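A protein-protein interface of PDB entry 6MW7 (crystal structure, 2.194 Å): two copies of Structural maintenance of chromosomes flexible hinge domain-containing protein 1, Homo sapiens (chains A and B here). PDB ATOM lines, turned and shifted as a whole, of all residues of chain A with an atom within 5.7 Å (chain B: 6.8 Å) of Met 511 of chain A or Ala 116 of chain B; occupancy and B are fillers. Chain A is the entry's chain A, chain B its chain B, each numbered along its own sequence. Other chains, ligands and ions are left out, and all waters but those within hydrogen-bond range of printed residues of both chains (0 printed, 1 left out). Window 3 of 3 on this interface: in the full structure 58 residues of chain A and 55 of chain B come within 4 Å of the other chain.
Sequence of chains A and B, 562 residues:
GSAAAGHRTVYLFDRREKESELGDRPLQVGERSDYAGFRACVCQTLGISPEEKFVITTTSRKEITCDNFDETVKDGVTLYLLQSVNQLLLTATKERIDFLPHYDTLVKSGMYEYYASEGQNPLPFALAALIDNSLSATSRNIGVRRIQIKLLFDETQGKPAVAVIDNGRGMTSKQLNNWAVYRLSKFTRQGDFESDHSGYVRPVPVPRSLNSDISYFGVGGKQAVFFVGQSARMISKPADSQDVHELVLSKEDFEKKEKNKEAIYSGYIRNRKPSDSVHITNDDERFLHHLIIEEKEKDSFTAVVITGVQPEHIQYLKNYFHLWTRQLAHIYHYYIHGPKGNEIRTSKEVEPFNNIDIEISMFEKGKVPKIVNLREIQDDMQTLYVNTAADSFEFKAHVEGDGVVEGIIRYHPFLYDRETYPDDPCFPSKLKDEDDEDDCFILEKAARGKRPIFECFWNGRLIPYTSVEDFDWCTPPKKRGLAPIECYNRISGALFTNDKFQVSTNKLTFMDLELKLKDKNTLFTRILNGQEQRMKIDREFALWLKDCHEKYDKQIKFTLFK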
ATOM      1  N   GLN A 502      17.970  13.434 -10.274  1.00  0.00           N
ATOM      2  CA  GLN A 502      19.016  13.906  -9.381  1.00  0.00           C
ATOM      3  C   GLN A 502      18.585  13.835  -7.923  1.00  0.00           C
ATOM      4  O   GLN A 502      17.412  14.017  -7.585  1.00  0.00           O
ATOM      5  CB  GLN A 502      19.397  15.348  -9.719  1.00  0.00           C
ATOM      6  CG  GLN A 502      20.039  15.524 -11.077  1.00  0.00           C
ATOM      7  CD  GLN A 502      20.374  16.970 -11.366  1.00  0.00           C
ATOM      8  OE1 GLN A 502      20.015  17.867 -10.602  1.00  0.00           O
ATOM      9  NE2 GLN A 502      21.068  17.208 -12.469  1.00  0.00           N
ATOM     10  N   VAL A 503      19.562  13.572  -7.056  1.00  0.00           N
ATOM     11  CA  VAL A 503      19.379  13.637  -5.615  1.00  0.00           C
ATOM     12  C   VAL A 503      20.346  14.670  -5.054  1.00  0.00           C
ATOM     13  O   VAL A 503      21.348  15.027  -5.678  1.00  0.00           O
ATOM     14  CB  VAL A 503      19.591  12.270  -4.934  1.00  0.00           C
ATOM     15  CG1 VAL A 503      18.511  11.291  -5.365  1.00  0.00           C
ATOM     16  CG2 VAL A 503      20.973  11.720  -5.253  1.00  0.00           C
ATOM     17  N   SER A 504      20.033  15.150  -3.855  1.00  0.00           N
ATOM     18  CA  SER A 504      20.919  16.080  -3.183  1.00  0.00           C
ATOM     19  C   SER A 504      22.200  15.361  -2.749  1.00  0.00           C
ATOM     20  O   SER A 504      22.288  14.130  -2.750  1.00  0.00           O
ATOM     21  CB  SER A 504      20.207  16.725  -1.992  1.00  0.00           C
ATOM     22  OG  SER A 504      19.847  15.766  -1.016  1.00  0.00           O
ATOM     23  N   THR A 509      17.289  13.623  -0.080  1.00  0.00           N
ATOM     24  CA  THR A 509      16.146  14.060  -0.869  1.00  0.00           C
ATOM     25  C   THR A 509      16.441  13.938  -2.356  1.00  0.00           C
ATOM     26  O   THR A 509      17.586  14.072  -2.792  1.00  0.00           O
ATOM     27  CB  THR A 509      15.770  15.521  -0.579  1.00  0.00           C
ATOM     28  OG1 THR A 509      16.929  16.353  -0.715  1.00  0.00           O
ATOM     29  CG2 THR A 509      15.189  15.675   0.814  1.00  0.00           C
ATOM     30  N   PHE A 510      15.389  13.680  -3.129  1.00  0.00           N
ATOM     31  CA  PHE A 510      15.421  13.962  -4.556  1.00  0.00           C
ATOM     32  C   PHE A 510      15.373  15.468  -4.782  1.00  0.00           C
ATOM     33  O   PHE A 510      14.813  16.218  -3.979  1.00  0.00           O
ATOM     34  CB  PHE A 510      14.239  13.310  -5.273  1.00  0.00           C
ATOM     35  CG  PHE A 510      14.406  11.838  -5.522  1.00  0.00           C
ATOM     36  CD1 PHE A 510      14.125  10.915  -4.530  1.00  0.00           C
ATOM     37  CD2 PHE A 510      14.821  11.378  -6.759  1.00  0.00           C
ATOM     38  CE1 PHE A 510      14.270   9.557  -4.762  1.00  0.00           C
ATOM     39  CE2 PHE A 510      14.968  10.021  -7.001  1.00  0.00           C
ATOM     40  CZ  PHE A 510      14.691   9.110  -6.000  1.00  0.00           C
ATOM     41  N   MET A 511      15.952  15.906  -5.894  1.00  0.00           N
ATOM     42  CA  MET A 511      15.970  17.325  -6.229  1.00  0.00           C
ATOM     43  C   MET A 511      14.613  17.807  -6.746  1.00  0.00           C
ATOM     44  O   MET A 511      14.130  18.861  -6.341  1.00  0.00           O
ATOM     45  CB  MET A 511      17.047  17.611  -7.273  1.00  0.00           C
ATOM     46  CG  MET A 511      18.474  17.384  -6.780  1.00  0.00           C
ATOM     47  SD  MET A 511      19.073  18.715  -5.479  1.00  0.00           S
ATOM     48  CE  MET A 511      19.130  20.266  -6.665  1.00  0.00           C
ATOM     49  N   ASP A 512      13.999  17.023  -7.633  1.00  0.00           N
ATOM     50  CA  ASP A 512      12.777  17.454  -8.304  1.00  0.00           C
ATOM     51  C   ASP A 512      11.971  16.277  -8.839  1.00  0.00           C
ATOM     52  O   ASP A 512      11.357  16.374  -9.907  1.00  0.00           O
ATOM     53  CB  ASP A 512      13.122  18.409  -9.451  1.00  0.00           C
ATOM     54  CG  ASP A 512      14.076  17.792 -10.465  1.00  0.00           C
ATOM     55  OD1 ASP A 512      14.358  16.580 -10.376  1.00  0.00           O
ATOM     56  OD2 ASP A 512      14.541  18.524 -11.360  1.00  0.00           O
ATOM     57  N   LEU A 513      11.946  15.167  -8.100  1.00  0.00           N
ATOM     58  CA  LEU A 513      11.313  13.954  -8.610  1.00  0.00           C
ATOM     59  C   LEU A 513       9.820  14.162  -8.838  1.00  0.00           C
ATOM     60  O   LEU A 513       9.308  13.917  -9.937  1.00  0.00           O
ATOM     61  CB  LEU A 513      11.561  12.796  -7.646  1.00  0.00           C
ATOM     62  CG  LEU A 513      10.855  11.475  -7.959  1.00  0.00           C
ATOM     63  CD1 LEU A 513      11.252  10.952  -9.331  1.00  0.00           C
ATOM     64  CD2 LEU A 513      11.166  10.449  -6.886  1.00  0.00           C
ATOM     65  N   LEU A 515       8.050  16.901  -9.044  1.00  0.00           N
ATOM     66  CA  LEU A 515       7.818  17.927 -10.054  1.00  0.00           C
ATOM     67  C   LEU A 515       7.847  17.339 -11.460  1.00  0.00           C
ATOM     68  O   LEU A 515       7.001  17.666 -12.298  1.00  0.00           O
ATOM     69  CB  LEU A 515       8.871  19.028  -9.909  1.00  0.00           C
ATOM     70  CG  LEU A 515       8.572  20.417 -10.466  1.00  0.00           C
ATOM     71  CD1 LEU A 515       7.365  21.036  -9.778  1.00  0.00           C
ATOM     72  CD2 LEU A 515       9.797  21.299 -10.294  1.00  0.00           C
ATOM     73  N   GLY B 110      26.972  24.253  -5.245  1.00  0.00           N
ATOM     74  CA  GLY B 110      25.554  24.543  -5.133  1.00  0.00           C
ATOM     75  C   GLY B 110      24.702  23.788  -6.132  1.00  0.00           C
ATOM     76  O   GLY B 110      23.509  24.066  -6.278  1.00  0.00           O
ATOM     77  N   MET B 111      25.298  22.824  -6.819  1.00  0.00           N
ATOM     78  CA  MET B 111      24.622  22.134  -7.909  1.00  0.00           C
ATOM     79  C   MET B 111      23.568  21.129  -7.433  1.00  0.00           C
ATOM     80  O   MET B 111      22.560  20.919  -8.108  1.00  0.00           O
ATOM     81  CB  MET B 111      25.654  21.418  -8.776  1.00  0.00           C
ATOM     82  CG  MET B 111      25.078  20.760 -10.006  1.00  0.00           C
ATOM     83  SD  MET B 111      26.489  20.141 -11.189  1.00  0.00           S
ATOM     84  CE  MET B 111      27.131  21.885 -11.803  1.00  0.00           C
ATOM     85  N   TYR B 112      23.801  20.506  -6.279  1.00  0.00           N
ATOM     86  CA  TYR B 112      22.904  19.482  -5.748  1.00  0.00           C
ATOM     87  C   TYR B 112      22.513  19.799  -4.312  1.00  0.00           C
ATOM     88  O   TYR B 112      22.440  18.910  -3.460  1.00  0.00           O
ATOM     89  CB  TYR B 112      23.544  18.097  -5.826  1.00  0.00           C
ATOM     90  CG  TYR B 112      24.076  17.729  -7.194  1.00  0.00           C
ATOM     91  CD1 TYR B 112      23.248  17.177  -8.162  1.00  0.00           C
ATOM     92  CD2 TYR B 112      25.413  17.920  -7.511  1.00  0.00           C
ATOM     93  CE1 TYR B 112      23.736  16.833  -9.410  1.00  0.00           C
ATOM     94  CE2 TYR B 112      25.910  17.581  -8.755  1.00  0.00           C
ATOM     95  CZ  TYR B 112      25.069  17.038  -9.701  1.00  0.00           C
ATOM     96  OH  TYR B 112      25.555  16.696 -10.942  1.00  0.00           O
ATOM     97  N   GLU B 113      22.251  21.070  -4.024  1.00  0.00           N
ATOM     98  CA  GLU B 113      21.925  21.512  -2.675  1.00  0.00           C
ATOM     99  C   GLU B 113      20.542  22.130  -2.549  1.00  0.00           C
ATOM    100  O   GLU B 113      19.935  22.025  -1.482  1.00  0.00           O
ATOM    101  CB  GLU B 113      22.959  22.538  -2.188  1.00  0.00           C
ATOM    102  CG  GLU B 113      24.400  22.079  -2.318  1.00  0.00           C
ATOM    103  CD  GLU B 113      24.718  20.891  -1.433  1.00  0.00           C
ATOM    104  OE1 GLU B 113      24.157  20.810  -0.318  1.00  0.00           O
ATOM    105  OE2 GLU B 113      25.525  20.038  -1.853  1.00  0.00           O
ATOM    106  N   TYR B 114      20.032  22.768  -3.601  1.00  0.00           N
ATOM    107  CA  TYR B 114      18.762  23.488  -3.543  1.00  0.00           C
ATOM    108  C   TYR B 114      17.673  22.611  -4.154  1.00  0.00           C
ATOM    109  O   TYR B 114      17.334  22.713  -5.332  1.00  0.00           O
ATOM    110  CB  TYR B 114      18.883  24.826  -4.262  1.00  0.00           C
ATOM    111  CG  TYR B 114      19.869  25.780  -3.632  1.00  0.00           C
ATOM    112  CD1 TYR B 114      19.623  26.345  -2.387  1.00  0.00           C
ATOM    113  CD2 TYR B 114      21.040  26.130  -4.289  1.00  0.00           C
ATOM    114  CE1 TYR B 114      20.522  27.224  -1.812  1.00  0.00           C
ATOM    115  CE2 TYR B 114      21.943  27.008  -3.722  1.00  0.00           C
ATOM    116  CZ  TYR B 114      21.680  27.553  -2.485  1.00  0.00           C
ATOM    117  OH  TYR B 114      22.579  28.428  -1.920  1.00  0.00           O
ATOM    118  N   TYR B 115      17.117  21.735  -3.323  1.00  0.00           N
ATOM    119  CA  TYR B 115      16.069  20.822  -3.752  1.00  0.00           C
ATOM    120  C   TYR B 115      14.701  21.474  -3.600  1.00  0.00           C
ATOM    121  O   TYR B 115      14.498  22.376  -2.786  1.00  0.00           O
ATOM    122  CB  TYR B 115      16.113  19.519  -2.949  1.00  0.00           C
ATOM    123  CG  TYR B 115      15.978  19.694  -1.451  1.00  0.00           C
ATOM    124  CD1 TYR B 115      17.091  19.933  -0.658  1.00  0.00           C
ATOM    125  CD2 TYR B 115      14.741  19.607  -0.829  1.00  0.00           C
ATOM    126  CE1 TYR B 115      16.977  20.090   0.710  1.00  0.00           C
ATOM    127  CE2 TYR B 115      14.616  19.764   0.541  1.00  0.00           C
ATOM    128  CZ  TYR B 115      15.739  20.005   1.306  1.00  0.00           C
ATOM    129  OH  TYR B 115      15.621  20.159   2.669  1.00  0.00           O
ATOM    130  N   ALA B 116      13.755  20.996  -4.402  1.00  0.00           N
ATOM    131  CA  ALA B 116      12.390  21.495  -4.345  1.00  0.00           C
ATOM    132  C   ALA B 116      11.612  20.768  -3.255  1.00  0.00           C
ATOM    133  O   ALA B 116      11.692  19.542  -3.136  1.00  0.00           O
ATOM    134  CB  ALA B 116      11.706  21.317  -5.696  1.00  0.00           C
ATOM    135  N   SER B 117      10.861  21.527  -2.460  1.00  0.00           N
ATOM    136  CA  SER B 117      10.021  20.948  -1.425  1.00  0.00           C
ATOM    137  C   SER B 117       8.789  21.821  -1.240  1.00  0.00           C
ATOM    138  O   SER B 117       8.850  23.045  -1.394  1.00  0.00           O
ATOM    139  CB  SER B 117      10.771  20.808  -0.095  1.00  0.00           C
ATOM    140  OG  SER B 117      10.083  19.942   0.792  1.00  0.00           O
ATOM    141  N   GLU B 118       7.670  21.174  -0.915  1.00  0.00           N
ATOM    142  CA  GLU B 118       6.423  21.871  -0.598  1.00  0.00           C
ATOM    143  C   GLU B 118       6.014  22.824  -1.720  1.00  0.00           C
ATOM    144  O   GLU B 118       5.455  23.896  -1.481  1.00  0.00           O
ATOM    145  CB  GLU B 118       6.550  22.616   0.733  1.00  0.00           C
ATOM    146  CG  GLU B 118       6.882  21.712   1.913  1.00  0.00           C
ATOM    147  CD  GLU B 118       7.634  22.435   3.013  1.00  0.00           C
ATOM    148  OE1 GLU B 118       7.507  23.675   3.102  1.00  0.00           O
ATOM    149  OE2 GLU B 118       8.356  21.766   3.784  1.00  0.00           O
ATOM    150  N   GLY B 119       6.294  22.428  -2.960  1.00  0.00           N
ATOM    151  CA  GLY B 119       5.862  23.191  -4.114  1.00  0.00           C
ATOM    152  C   GLY B 119       6.648  24.452  -4.400  1.00  0.00           C
ATOM    153  O   GLY B 119       6.255  25.215  -5.289  1.00  0.00           O
ATOM    154  N   GLN B 120       7.744  24.701  -3.686  1.00  0.00           N
ATOM    155  CA  GLN B 120       8.526  25.914  -3.879  1.00  0.00           C
ATOM    156  C   GLN B 120       9.670  25.673  -4.853  1.00  0.00           C
ATOM    157  O   GLN B 120      10.352  24.647  -4.788  1.00  0.00           O
ATOM    158  CB  GLN B 120       9.095  26.414  -2.551  1.00  0.00           C
ATOM    159  CG  GLN B 120       8.065  26.627  -1.457  1.00  0.00           C
ATOM    160  CD  GLN B 120       8.689  27.128  -0.167  1.00  0.00           C
ATOM    161  OE1 GLN B 120       9.315  28.188  -0.138  1.00  0.00           O
ATOM    162  NE2 GLN B 120       8.533  26.360   0.907  1.00  0.00           N
ATOM    163  N   ASN B 121       9.872  26.623  -5.757  1.00  0.00           N
ATOM    164  CA  ASN B 121      11.086  26.628  -6.562  1.00  0.00           C
ATOM    165  C   ASN B 121      12.232  27.167  -5.712  1.00  0.00           C
ATOM    166  O   ASN B 121      12.101  28.245  -5.126  1.00  0.00           O
ATOM    167  CB  ASN B 121      10.910  27.488  -7.810  1.00  0.00           C
ATOM    168  CG  ASN B 121      12.074  27.360  -8.775  1.00  0.00           C
ATOM    169  OD1 ASN B 121      13.236  27.406  -8.376  1.00  0.00           O
ATOM    170  ND2 ASN B 121      11.765  27.187 -10.054  1.00  0.00           N
ATOM    171  N   PRO B 122      13.353  26.453  -5.602  1.00  0.00           N
ATOM    172  CA  PRO B 122      14.403  26.863  -4.661  1.00  0.00           C
ATOM    173  C   PRO B 122      15.394  27.895  -5.180  1.00  0.00           C
ATOM    174  O   PRO B 122      16.301  28.273  -4.432  1.00  0.00           O
ATOM    175  CB  PRO B 122      15.113  25.534  -4.373  1.00  0.00           C
ATOM    176  CG  PRO B 122      14.995  24.778  -5.645  1.00  0.00           C
ATOM    177  CD  PRO B 122      13.662  25.161  -6.239  1.00  0.00           C
ATOM    178  N   PHE B 125      16.246  30.885  -2.956  1.00  0.00           N
ATOM    179  CA  PHE B 125      17.047  30.646  -1.759  1.00  0.00           C
ATOM    180  C   PHE B 125      18.522  30.924  -2.016  1.00  0.00           C
ATOM    181  O   PHE B 125      19.246  31.322  -1.098  1.00  0.00           O
ATOM    182  CB  PHE B 125      16.856  29.211  -1.263  1.00  0.00           C
ATOM    183  CG  PHE B 125      15.416  28.820  -1.061  1.00  0.00           C
ATOM    184  CD1 PHE B 125      14.480  29.748  -0.636  1.00  0.00           C
ATOM    185  CD2 PHE B 125      15.001  27.521  -1.301  1.00  0.00           C
ATOM    186  CE1 PHE B 125      13.157  29.387  -0.450  1.00  0.00           C
ATOM    187  CE2 PHE B 125      13.679  27.153  -1.119  1.00  0.00           C
ATOM    188  CZ  PHE B 125      12.756  28.088  -0.694  1.00  0.00           C
ATOM    189  N   PHE B 227      25.560  27.818  -8.138  1.00  0.00           N
ATOM    190  CA  PHE B 227      24.238  27.321  -8.507  1.00  0.00           C
ATOM    191  C   PHE B 227      23.643  28.156  -9.636  1.00  0.00           C
ATOM    192  O   PHE B 227      23.174  27.615 -10.646  1.00  0.00           O
ATOM    193  CB  PHE B 227      23.310  27.337  -7.288  1.00  0.00           C
ATOM    194  CG  PHE B 227      21.882  26.990  -7.608  1.00  0.00           C
ATOM    195  CD1 PHE B 227      21.538  25.708  -7.999  1.00  0.00           C
ATOM    196  CD2 PHE B 227      20.885  27.944  -7.514  1.00  0.00           C
ATOM    197  CE1 PHE B 227      20.227  25.386  -8.296  1.00  0.00           C
ATOM    198  CE2 PHE B 227      19.570  27.626  -7.808  1.00  0.00           C
ATOM    199  CZ  PHE B 227      19.243  26.346  -8.198  1.00  0.00           C
ATOM    200  N   TYR B 465      12.091  25.369   4.745  1.00  0.00           N
ATOM    201  CA  TYR B 465      11.624  23.985   4.753  1.00  0.00           C
ATOM    202  C   TYR B 465      11.462  23.408   6.156  1.00  0.00           C
ATOM    203  O   TYR B 465      11.333  22.187   6.300  1.00  0.00           O
ATOM    204  CB  TYR B 465      12.571  23.105   3.933  1.00  0.00           C
ATOM    205  CG  TYR B 465      12.561  23.377   2.440  1.00  0.00           C
ATOM    206  CD1 TYR B 465      11.539  24.110   1.847  1.00  0.00           C
ATOM    207  CD2 TYR B 465      13.572  22.888   1.621  1.00  0.00           C
ATOM    208  CE1 TYR B 465      11.530  24.352   0.485  1.00  0.00           C
ATOM    209  CE2 TYR B 465      13.570  23.124   0.260  1.00  0.00           C
ATOM    210  CZ  TYR B 465      12.548  23.855  -0.304  1.00  0.00           C
ATOM    211  OH  TYR B 465      12.553  24.084  -1.662  1.00  0.00           O
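Gln 502 of chain A touches Tyr 112 of chain B.
Tyr 112 of chain B touches Val 503 of chain A (CB to O, 3.8 Å).
Ser 504 of chain A touches Tyr 112 of chain B (CA to O, 3.2 Å).
Thr 509 of chain A touches Tyr 115 of chain B (OG1 to CG, 3.6 Å).
O of Phe 510 of chain A touches CB of Tyr 115 of chain B, at 3.7 Å.
Met 511 of chain A touches Met 111 of chain B (CE to O, 3.8 Å).
Met 511 of chain A touches Tyr 112 of chain B.
Met 511 of chain A touches Tyr 114 of chain B.
Met 511 of chain A touches Tyr 115 of chain B (O to CA, 3.8 Å).
N of Ala 116 of chain B sits at hydrogen-bond distance from O of Met 511 of chain A, at 2.9 Å.
Of the 9 printed residues of chain A, 6 touch a printed residue of chain B.
Printed residues of chain A that touch a printed residue of chain B: Gln 502, Val 503, Ser 504, Thr 509, Phe 510 and Met 511.
Hydrophobic or aromatic side chains of chain A that line the printed part of chain B: Met 511.
Along chain A the printed residues that touch a printed residue of chain B span positions 502 to 511.
Hydrophobic or aromatic side chains of chain B within 4 Å of the printed part of chain A: Tyr 112, Tyr 115 and Ala 116.
Among the printed residues, no Asp or Glu carboxylate lies within 4 Å of a Lys or Arg side-chain nitrogen of the other chain.
O of Tyr 115 of chain B lies within hydrogen-bond range of OH of Tyr 465 of chain B.
The backbone carbonyl oxygen (O) of Thr 509 of chain A sits at hydrogen-bond distance from the backbone NH (N) of Ser 504 of chain A (2.9 Å).
OH of Tyr 112 of chain B is in hydrogen-bond range of SD of Met 111 of chain B (3.6 Å).
O of Gln 502 of chain A sits at hydrogen-bond distance from N of Met 511 of chain A.
No position is printed for both chains.
Ala 116 of chain B touches one residue of chain A.
Of the printed residues of chain B, Thr 509 of chain A touches Tyr 115.
Of the printed residues of chain B, Gln 502 of chain A touches Tyr 112.
Printed residues of chain B within 4 Å of Ser 504 of chain A: Tyr 112.
The nearest residue of chain A that does not touch Ala 116 of chain B is Phe 510 of chain A (4.6 Å).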
